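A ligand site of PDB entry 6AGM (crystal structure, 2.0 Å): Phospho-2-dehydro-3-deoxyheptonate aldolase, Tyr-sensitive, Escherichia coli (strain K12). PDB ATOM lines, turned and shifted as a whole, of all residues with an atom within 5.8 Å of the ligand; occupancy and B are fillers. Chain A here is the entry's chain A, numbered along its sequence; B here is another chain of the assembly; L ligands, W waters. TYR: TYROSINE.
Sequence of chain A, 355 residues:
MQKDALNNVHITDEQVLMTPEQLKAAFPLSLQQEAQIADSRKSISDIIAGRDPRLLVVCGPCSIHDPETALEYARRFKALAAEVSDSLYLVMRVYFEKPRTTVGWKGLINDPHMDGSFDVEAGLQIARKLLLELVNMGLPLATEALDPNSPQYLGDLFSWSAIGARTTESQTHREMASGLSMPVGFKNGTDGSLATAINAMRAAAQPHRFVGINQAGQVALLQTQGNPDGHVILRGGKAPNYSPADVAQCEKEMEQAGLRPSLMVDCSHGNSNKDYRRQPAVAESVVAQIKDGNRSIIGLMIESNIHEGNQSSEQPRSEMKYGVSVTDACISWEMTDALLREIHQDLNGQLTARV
The side-chain amide oxygen (OE1) of Gln 152 is in hydrogen-bond range of a nitrogen (N) of the ligand (2.8 Å). OH of the ligand lies within hydrogen-bond range of O of Pro 148, at 2.5 Å. OXT of the ligand is in hydrogen-bond range of OG of Ser 181 (2.6 Å). The backbone NH of Ile 213 sits at hydrogen-bond distance from an oxygen (OH) of the ligand, at 3.2 Å. A nitrogen (N) of the ligand sits at hydrogen-bond distance from the side-chain amide oxygen of Asn 8 of chain B (3.0 Å). N of Asn 8 of chain B sits at hydrogen-bond distance from OXT of the ligand. N of Ser 181 sits at hydrogen-bond distance from O of the ligand (3.0 Å).
O of Ile 213 sits at hydrogen-bond distance from NE2 of Gln 152, at 2.7 Å. O of Leu 6 of chain B sits close to OG of Ser 181 (3.2 Å). The side-chain amino group (NZ) of Lys 24 lies close to the backbone carbonyl oxygen (O) of Gln 152 (3.4 Å). N of Asn 8 of chain B is in hydrogen-bond range of OG of Ser 181, 3.4 Å away. The side-chain amide nitrogen (ND2) of Asn 7 of chain B lies close to the side-chain amino group (NZ) of Lys 24 (3.0 Å). The backbone carbonyl oxygen of Leu 6 of chain B sits at hydrogen-bond distance from the guanidinium group of Arg 41, at 2.9 Å. The side-chain hydroxyl (OG) of Ser 181 sits at hydrogen-bond distance from the backbone NH (N) of Val 9 of chain B, at 3.1 Å. N of Leu 222 lies within hydrogen-bond range of O of Phe 210 (2.9 Å).
Pro 151 touches the ligand (CB to CD2, 3.6 Å). O of Gly 179 touches CB of the ligand, 3.5 Å away. Leu 180 touches the ligand (CA to O, 3.6 Å). CE1 of Phe 210 touches CZ of the ligand, 3.7 Å away. Gly 212 touches the ligand. Leu 222 touches the ligand (CD2 to CE1, 3.5 Å). Leu 6 of chain B touches the ligand. Asn 7 of chain B touches the ligand. Hydrophobic or aromatic side chains within 4 Å of the ligand: Pro 151, Leu 180, Phe 210 and Leu 222. 13 residues have an atom within 4 Å of the ligand: Pro 148, Pro 151, Gln 152, Gly 179, Leu 180, Ser 181, Phe 210, Gly 212, Ile 213, Leu 222, Leu 6 of chain B, Asn 7 of chain B and Asn 8 of chain B.
Water W3 lies within hydrogen-bond range of a nitrogen (N) of the ligand (3.0 Å), the backbone carbonyl oxygen (O) of Pro 151 (3.3 Å) and the side-chain amide nitrogen (ND2) of Asn 7 of chain B (3.4 Å). Water W1 lies within hydrogen-bond range of the backbone carbonyl oxygen of Leu 6 of chain B, the guanidinium group of Arg 41, an oxygen (OXT) of the ligand and the backbone carbonyl oxygen of Gly 155. Water W2 lies within hydrogen-bond range of O of Gly 179 (2.5 Å), OG of Ser 181 (2.7 Å), N of Val 9 of chain B (3.2 Å) and OXT of the ligand (3.5 Å).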
ATOM      1  N   LYS A  24      23.253 -29.789  -7.047  1.00  0.00           N
ATOM      2  CA  LYS A  24      22.419 -30.593  -7.944  1.00  0.00           C
ATOM      3  C   LYS A  24      22.318 -32.037  -7.485  1.00  0.00           C
ATOM      4  O   LYS A  24      21.299 -32.694  -7.730  1.00  0.00           O
ATOM      5  CB  LYS A  24      22.960 -30.511  -9.370  1.00  0.00           C
ATOM      6  CG  LYS A  24      22.925 -29.113  -9.950  1.00  0.00           C
ATOM      7  CD  LYS A  24      23.481 -29.083 -11.354  1.00  0.00           C
ATOM      8  CE  LYS A  24      23.232 -27.739 -12.016  1.00  0.00           C
ATOM      9  NZ  LYS A  24      23.743 -27.727 -13.410  1.00  0.00           N
ATOM     10  N   ARG A  41      11.880 -24.698 -23.304  1.00  0.00           N
ATOM     11  CA  ARG A  41      12.931 -23.962 -24.001  1.00  0.00           C
ATOM     12  C   ARG A  41      12.725 -24.004 -25.510  1.00  0.00           C
ATOM     13  O   ARG A  41      12.862 -22.982 -26.196  1.00  0.00           O
ATOM     14  CB  ARG A  41      14.311 -24.535 -23.644  1.00  0.00           C
ATOM     15  CG  ARG A  41      14.775 -24.252 -22.213  1.00  0.00           C
ATOM     16  CD  ARG A  41      16.119 -24.918 -21.919  1.00  0.00           C
ATOM     17  NE  ARG A  41      16.628 -24.556 -20.600  1.00  0.00           N
ATOM     18  CZ  ARG A  41      17.797 -24.968 -20.111  1.00  0.00           C
ATOM     19  NH1 ARG A  41      18.586 -25.767 -20.810  1.00  0.00           N
ATOM     20  NH2 ARG A  41      18.169 -24.578 -18.893  1.00  0.00           N
ATOM     21  N   PRO A 148      28.180 -14.672 -13.340  1.00  0.00           N
ATOM     22  CA  PRO A 148      28.627 -15.861 -14.085  1.00  0.00           C
ATOM     23  C   PRO A 148      28.493 -17.173 -13.326  1.00  0.00           C
ATOM     24  O   PRO A 148      28.701 -18.232 -13.932  1.00  0.00           O
ATOM     25  CB  PRO A 148      30.108 -15.552 -14.376  1.00  0.00           C
ATOM     26  CG  PRO A 148      30.325 -14.118 -13.950  1.00  0.00           C
ATOM     27  CD  PRO A 148      29.312 -13.844 -12.902  1.00  0.00           C
ATOM     28  N   ASN A 149      28.171 -17.142 -12.036  1.00  0.00           N
ATOM     29  CA  ASN A 149      28.108 -18.352 -11.216  1.00  0.00           C
ATOM     30  C   ASN A 149      26.699 -18.884 -11.010  1.00  0.00           C
ATOM     31  O   ASN A 149      26.494 -20.096 -11.007  1.00  0.00           O
ATOM     32  CB  ASN A 149      28.750 -18.099  -9.841  1.00  0.00           C
ATOM     33  CG  ASN A 149      30.154 -17.522  -9.949  1.00  0.00           C
ATOM     34  OD1 ASN A 149      30.661 -17.298 -11.056  1.00  0.00           O
ATOM     35  ND2 ASN A 149      30.784 -17.273  -8.810  1.00  0.00           N
ATOM     36  N   PRO A 151      24.135 -19.131 -13.006  1.00  0.00           N
ATOM     37  CA  PRO A 151      23.679 -20.113 -14.013  1.00  0.00           C
ATOM     38  C   PRO A 151      24.176 -21.518 -13.729  1.00  0.00           C
ATOM     39  O   PRO A 151      23.395 -22.457 -13.893  1.00  0.00           O
ATOM     40  CB  PRO A 151      24.229 -19.544 -15.322  1.00  0.00           C
ATOM     41  CG  PRO A 151      24.270 -18.079 -15.094  1.00  0.00           C
ATOM     42  CD  PRO A 151      24.699 -17.935 -13.655  1.00  0.00           C
ATOM     43  N   GLN A 152      25.392 -21.688 -13.236  1.00  0.00           N
ATOM     44  CA  GLN A 152      25.860 -23.048 -12.925  1.00  0.00           C
ATOM     45  C   GLN A 152      25.051 -23.663 -11.798  1.00  0.00           C
ATOM     46  O   GLN A 152      24.795 -24.874 -11.800  1.00  0.00           O
ATOM     47  CB  GLN A 152      27.341 -23.015 -12.566  1.00  0.00           C
ATOM     48  CG  GLN A 152      28.264 -22.786 -13.742  1.00  0.00           C
ATOM     49  CD  GLN A 152      28.399 -24.011 -14.624  1.00  0.00           C
ATOM     50  OE1 GLN A 152      27.422 -24.514 -15.183  1.00  0.00           O
ATOM     51  NE2 GLN A 152      29.626 -24.513 -14.759  1.00  0.00           N
ATOM     52  N   GLY A 155      20.637 -22.577 -13.376  1.00  0.00           N
ATOM     53  CA  GLY A 155      20.143 -22.315 -14.711  1.00  0.00           C
ATOM     54  C   GLY A 155      19.481 -23.495 -15.364  1.00  0.00           C
ATOM     55  O   GLY A 155      18.640 -23.305 -16.249  1.00  0.00           O
ATOM     56  N   MET A 176      28.804 -14.273 -22.123  1.00  0.00           N
ATOM     57  CA  MET A 176      28.229 -15.428 -21.430  1.00  0.00           C
ATOM     58  C   MET A 176      26.965 -15.935 -22.122  1.00  0.00           C
ATOM     59  O   MET A 176      26.703 -17.142 -22.106  1.00  0.00           O
ATOM     60  CB  MET A 176      27.938 -15.072 -19.973  1.00  0.00           C
ATOM     61  CG  MET A 176      27.475 -16.252 -19.147  1.00  0.00           C
ATOM     62  SD  MET A 176      27.205 -15.828 -17.417  1.00  0.00           S
ATOM     63  CE  MET A 176      25.966 -14.535 -17.583  1.00  0.00           C
ATOM     64  N   GLY A 179      26.923 -18.886 -24.403  1.00  0.00           N
ATOM     65  CA  GLY A 179      27.148 -20.189 -23.828  1.00  0.00           C
ATOM     66  C   GLY A 179      26.014 -20.655 -22.930  1.00  0.00           C
ATOM     67  O   GLY A 179      26.140 -21.677 -22.255  1.00  0.00           O
ATOM     68  N   LEU A 180      24.909 -19.917 -22.914  1.00  0.00           N
ATOM     69  CA  LEU A 180      23.761 -20.298 -22.106  1.00  0.00           C
ATOM     70  C   LEU A 180      22.851 -21.221 -22.895  1.00  0.00           C
ATOM     71  O   LEU A 180      22.675 -21.053 -24.105  1.00  0.00           O
ATOM     72  CB  LEU A 180      22.989 -19.069 -21.639  1.00  0.00           C
ATOM     73  CG  LEU A 180      23.713 -18.108 -20.693  1.00  0.00           C
ATOM     74  CD1 LEU A 180      22.829 -16.904 -20.363  1.00  0.00           C
ATOM     75  CD2 LEU A 180      24.150 -18.816 -19.411  1.00  0.00           C
ATOM     76  N   SER A 181      22.268 -22.204 -22.206  1.00  0.00           N
ATOM     77  CA  SER A 181      21.455 -23.230 -22.845  1.00  0.00           C
ATOM     78  C   SER A 181      20.004 -22.821 -23.064  1.00  0.00           C
ATOM     79  O   SER A 181      19.220 -23.633 -23.552  1.00  0.00           O
ATOM     80  CB  SER A 181      21.500 -24.523 -22.021  1.00  0.00           C
ATOM     81  OG  SER A 181      22.835 -24.947 -21.784  1.00  0.00           O
ATOM     82  N   MET A 182      19.626 -21.604 -22.713  1.00  0.00           N
ATOM     83  CA  MET A 182      18.251 -21.149 -22.830  1.00  0.00           C
ATOM     84  C   MET A 182      18.171 -19.933 -23.749  1.00  0.00           C
ATOM     85  O   MET A 182      19.167 -19.232 -23.972  1.00  0.00           O
ATOM     86  CB  MET A 182      17.671 -20.790 -21.454  1.00  0.00           C
ATOM     87  CG  MET A 182      18.230 -19.498 -20.859  1.00  0.00           C
ATOM     88  SD  MET A 182      19.728 -19.760 -19.894  1.00  0.00           S
ATOM     89  CE  MET A 182      19.214 -21.037 -18.753  1.00  0.00           C
ATOM     90  N   PHE A 210      34.427 -17.075 -22.203  1.00  0.00           N
ATOM     91  CA  PHE A 210      34.170 -16.232 -21.034  1.00  0.00           C
ATOM     92  C   PHE A 210      34.695 -16.915 -19.782  1.00  0.00           C
ATOM     93  O   PHE A 210      34.808 -18.139 -19.718  1.00  0.00           O
ATOM     94  CB  PHE A 210      32.678 -15.881 -20.888  1.00  0.00           C
ATOM     95  CG  PHE A 210      31.806 -17.021 -20.430  1.00  0.00           C
ATOM     96  CD1 PHE A 210      31.449 -17.159 -19.096  1.00  0.00           C
ATOM     97  CD2 PHE A 210      31.313 -17.948 -21.339  1.00  0.00           C
ATOM     98  CE1 PHE A 210      30.627 -18.194 -18.678  1.00  0.00           C
ATOM     99  CE2 PHE A 210      30.493 -18.983 -20.931  1.00  0.00           C
ATOM    100  CZ  PHE A 210      30.156 -19.112 -19.592  1.00  0.00           C
ATOM    101  N   VAL A 211      35.011 -16.103 -18.775  1.00  0.00           N
ATOM    102  CA  VAL A 211      35.443 -16.607 -17.470  1.00  0.00           C
ATOM    103  C   VAL A 211      34.216 -16.857 -16.609  1.00  0.00           C
ATOM    104  O   VAL A 211      33.374 -15.960 -16.426  1.00  0.00           O
ATOM    105  CB  VAL A 211      36.407 -15.625 -16.789  1.00  0.00           C
ATOM    106  CG1 VAL A 211      36.786 -16.134 -15.405  1.00  0.00           C
ATOM    107  CG2 VAL A 211      37.648 -15.424 -17.650  1.00  0.00           C
ATOM    108  N   GLY A 212      34.100 -18.069 -16.081  1.00  0.00           N
ATOM    109  CA  GLY A 212      33.045 -18.411 -15.132  1.00  0.00           C
ATOM    110  C   GLY A 212      33.558 -19.435 -14.154  1.00  0.00           C
ATOM    111  O   GLY A 212      34.718 -19.377 -13.730  1.00  0.00           O
ATOM    112  N   ILE A 213      32.713 -20.406 -13.815  1.00  0.00           N
ATOM    113  CA  ILE A 213      33.119 -21.511 -12.966  1.00  0.00           C
ATOM    114  C   ILE A 213      32.653 -22.820 -13.593  1.00  0.00           C
ATOM    115  O   ILE A 213      31.681 -22.846 -14.364  1.00  0.00           O
ATOM    116  CB  ILE A 213      32.565 -21.382 -11.520  1.00  0.00           C
ATOM    117  CG1 ILE A 213      31.032 -21.390 -11.519  1.00  0.00           C
ATOM    118  CG2 ILE A 213      33.111 -20.128 -10.839  1.00  0.00           C
ATOM    119  CD1 ILE A 213      30.425 -21.505 -10.130  1.00  0.00           C
ATOM    120  N   ASN A 214      33.354 -23.905 -13.267  1.00  0.00           N
ATOM    121  CA  ASN A 214      32.912 -25.232 -13.662  1.00  0.00           C
ATOM    122  C   ASN A 214      31.935 -25.784 -12.628  1.00  0.00           C
ATOM    123  O   ASN A 214      31.582 -25.111 -11.657  1.00  0.00           O
ATOM    124  CB  ASN A 214      34.112 -26.161 -13.886  1.00  0.00           C
ATOM    125  CG  ASN A 214      34.945 -26.398 -12.627  1.00  0.00           C
ATOM    126  OD1 ASN A 214      34.555 -26.042 -11.509  1.00  0.00           O
ATOM    127  ND2 ASN A 214      36.112 -27.013 -12.809  1.00  0.00           N
ATOM    128  N   GLN A 215      31.487 -27.015 -12.826  1.00  0.00           N
ATOM    129  CA  GLN A 215      30.543 -27.618 -11.902  1.00  0.00           C
ATOM    130  C   GLN A 215      31.158 -27.900 -10.538  1.00  0.00           C
ATOM    131  O   GLN A 215      30.434 -28.146  -9.571  1.00  0.00           O
ATOM    132  CB  GLN A 215      29.961 -28.903 -12.496  1.00  0.00           C
ATOM    133  CG  GLN A 215      28.825 -28.664 -13.491  1.00  0.00           C
ATOM    134  CD  GLN A 215      27.503 -28.313 -12.815  1.00  0.00           C
ATOM    135  OE1 GLN A 215      26.972 -29.095 -12.022  1.00  0.00           O
ATOM    136  NE2 GLN A 215      26.972 -27.132 -13.132  1.00  0.00           N
ATOM    137  N   LEU A 222      35.450 -20.886 -20.244  1.00  0.00           N
ATOM    138  CA  LEU A 222      34.474 -21.645 -21.012  1.00  0.00           C
ATOM    139  C   LEU A 222      34.484 -21.176 -22.458  1.00  0.00           C
ATOM    140  O   LEU A 222      34.450 -19.978 -22.725  1.00  0.00           O
ATOM    141  CB  LEU A 222      33.082 -21.499 -20.405  1.00  0.00           C
ATOM    142  CG  LEU A 222      33.069 -22.004 -18.955  1.00  0.00           C
ATOM    143  CD1 LEU A 222      32.914 -20.851 -17.975  1.00  0.00           C
ATOM    144  CD2 LEU A 222      32.003 -23.054 -18.761  1.00  0.00           C
ATOM    145  N   LEU B   6      19.983 -30.335 -20.925  1.00  0.00           N
ATOM    146  CA  LEU B   6      19.779 -29.013 -20.333  1.00  0.00           C
ATOM    147  C   LEU B   6      21.065 -28.264 -20.026  1.00  0.00           C
ATOM    148  O   LEU B   6      21.061 -27.039 -20.055  1.00  0.00           O
ATOM    149  CB  LEU B   6      18.976 -29.145 -19.026  1.00  0.00           C
ATOM    150  CG  LEU B   6      17.536 -29.637 -19.088  1.00  0.00           C
ATOM    151  CD1 LEU B   6      16.899 -29.549 -17.716  1.00  0.00           C
ATOM    152  CD2 LEU B   6      16.737 -28.855 -20.114  1.00  0.00           C
ATOM    153  N   ASN B   7      22.159 -28.965 -19.722  1.00  0.00           N
ATOM    154  CA  ASN B   7      23.375 -28.349 -19.218  1.00  0.00           C
ATOM    155  C   ASN B   7      24.444 -28.308 -20.302  1.00  0.00           C
ATOM    156  O   ASN B   7      24.684 -29.305 -20.991  1.00  0.00           O
ATOM    157  CB  ASN B   7      23.900 -29.094 -17.989  1.00  0.00           C
ATOM    158  CG  ASN B   7      22.841 -29.281 -16.924  1.00  0.00           C
ATOM    159  OD1 ASN B   7      22.249 -30.348 -16.789  1.00  0.00           O
ATOM    160  ND2 ASN B   7      22.601 -28.228 -16.159  1.00  0.00           N
ATOM    161  N   ASN B   8      25.082 -27.136 -20.438  1.00  0.00           N
ATOM    162  CA  ASN B   8      26.211 -26.945 -21.343  1.00  0.00           C
ATOM    163  C   ASN B   8      25.872 -27.324 -22.774  1.00  0.00           C
ATOM    164  O   ASN B   8      26.715 -27.857 -23.503  1.00  0.00           O
ATOM    165  CB  ASN B   8      27.452 -27.704 -20.857  1.00  0.00           C
ATOM    166  CG  ASN B   8      28.033 -27.113 -19.589  1.00  0.00           C
ATOM    167  OD1 ASN B   8      27.419 -26.239 -18.960  1.00  0.00           O
ATOM    168  ND2 ASN B   8      29.215 -27.576 -19.194  1.00  0.00           N
ATOM    169  N   VAL B   9      24.633 -27.070 -23.180  1.00  0.00           N
ATOM    170  CA  VAL B   9      24.211 -27.341 -24.558  1.00  0.00           C
ATOM    171  C   VAL B   9      25.054 -26.526 -25.542  1.00  0.00           C
ATOM    172  O   VAL B   9      25.364 -26.987 -26.640  1.00  0.00           O
ATOM    173  CB  VAL B   9      22.710 -27.064 -24.722  1.00  0.00           C
ATOM    174  CG1 VAL B   9      22.275 -27.252 -26.167  1.00  0.00           C
ATOM    175  CG2 VAL B   9      21.907 -27.954 -23.788  1.00  0.00           C
ATOM    176  N   ILE B  11      28.151 -25.112 -24.751  1.00  0.00           N
ATOM    177  CA  ILE B  11      29.532 -25.053 -24.268  1.00  0.00           C
ATOM    178  C   ILE B  11      30.275 -26.231 -24.888  1.00  0.00           C
ATOM    179  O   ILE B  11      29.872 -27.384 -24.723  1.00  0.00           O
ATOM    180  CB  ILE B  11      29.617 -25.111 -22.731  1.00  0.00           C
ATOM    181  CG1 ILE B  11      28.804 -23.981 -22.104  1.00  0.00           C
ATOM    182  CG2 ILE B  11      31.080 -25.048 -22.275  1.00  0.00           C
ATOM    183  CD1 ILE B  11      29.436 -22.615 -22.236  1.00  0.00           C
ATOM    184  N   GLU B  14      35.860 -26.585 -21.588  1.00  0.00           N
ATOM    185  CA  GLU B  14      35.964 -25.987 -20.271  1.00  0.00           C
ATOM    186  C   GLU B  14      37.381 -26.213 -19.749  1.00  0.00           C
ATOM    187  O   GLU B  14      37.878 -27.338 -19.820  1.00  0.00           O
ATOM    188  CB  GLU B  14      34.923 -26.581 -19.326  1.00  0.00           C
ATOM    189  CG  GLU B  14      34.831 -25.922 -17.974  1.00  0.00           C
ATOM    190  CD  GLU B  14      33.641 -26.434 -17.193  1.00  0.00           C
ATOM    191  OE1 GLU B  14      32.775 -25.616 -16.816  1.00  0.00           O
ATOM    192  OE2 GLU B  14      33.562 -27.654 -16.958  1.00  0.00           O
HETATM  193  N   TYR L   1      25.714 -24.311 -17.360  1.00  0.00           N
HETATM  194  CA  TYR L   1      25.238 -23.151 -18.101  1.00  0.00           C
HETATM  195  C   TYR L   1      24.139 -23.538 -19.075  1.00  0.00           C
HETATM  196  O   TYR L   1      23.352 -22.693 -19.501  1.00  0.00           O
HETATM  197  CB  TYR L   1      26.399 -22.480 -18.860  1.00  0.00           C
HETATM  198  CG  TYR L   1      27.373 -21.774 -17.937  1.00  0.00           C
HETATM  199  CD1 TYR L   1      28.603 -22.340 -17.629  1.00  0.00           C
HETATM  200  CD2 TYR L   1      27.056 -20.552 -17.367  1.00  0.00           C
HETATM  201  CE1 TYR L   1      29.490 -21.711 -16.777  1.00  0.00           C
HETATM  202  CE2 TYR L   1      27.931 -19.902 -16.511  1.00  0.00           C
HETATM  203  CZ  TYR L   1      29.149 -20.494 -16.225  1.00  0.00           C
HETATM  204  OH  TYR L   1      30.028 -19.859 -15.375  1.00  0.00           O
HETATM  205  OXT TYR L   1      23.995 -24.706 -19.449  1.00  0.00           O
HETATM  206  O   HOH W   1      21.083 -24.779 -18.163  1.00  0.00           O
HETATM  207  O   HOH W   2      25.187 -23.955 -22.642  1.00  0.00           O
HETATM  208  O   HOH W   3      23.026 -24.823 -16.197  1.00  0.00           O
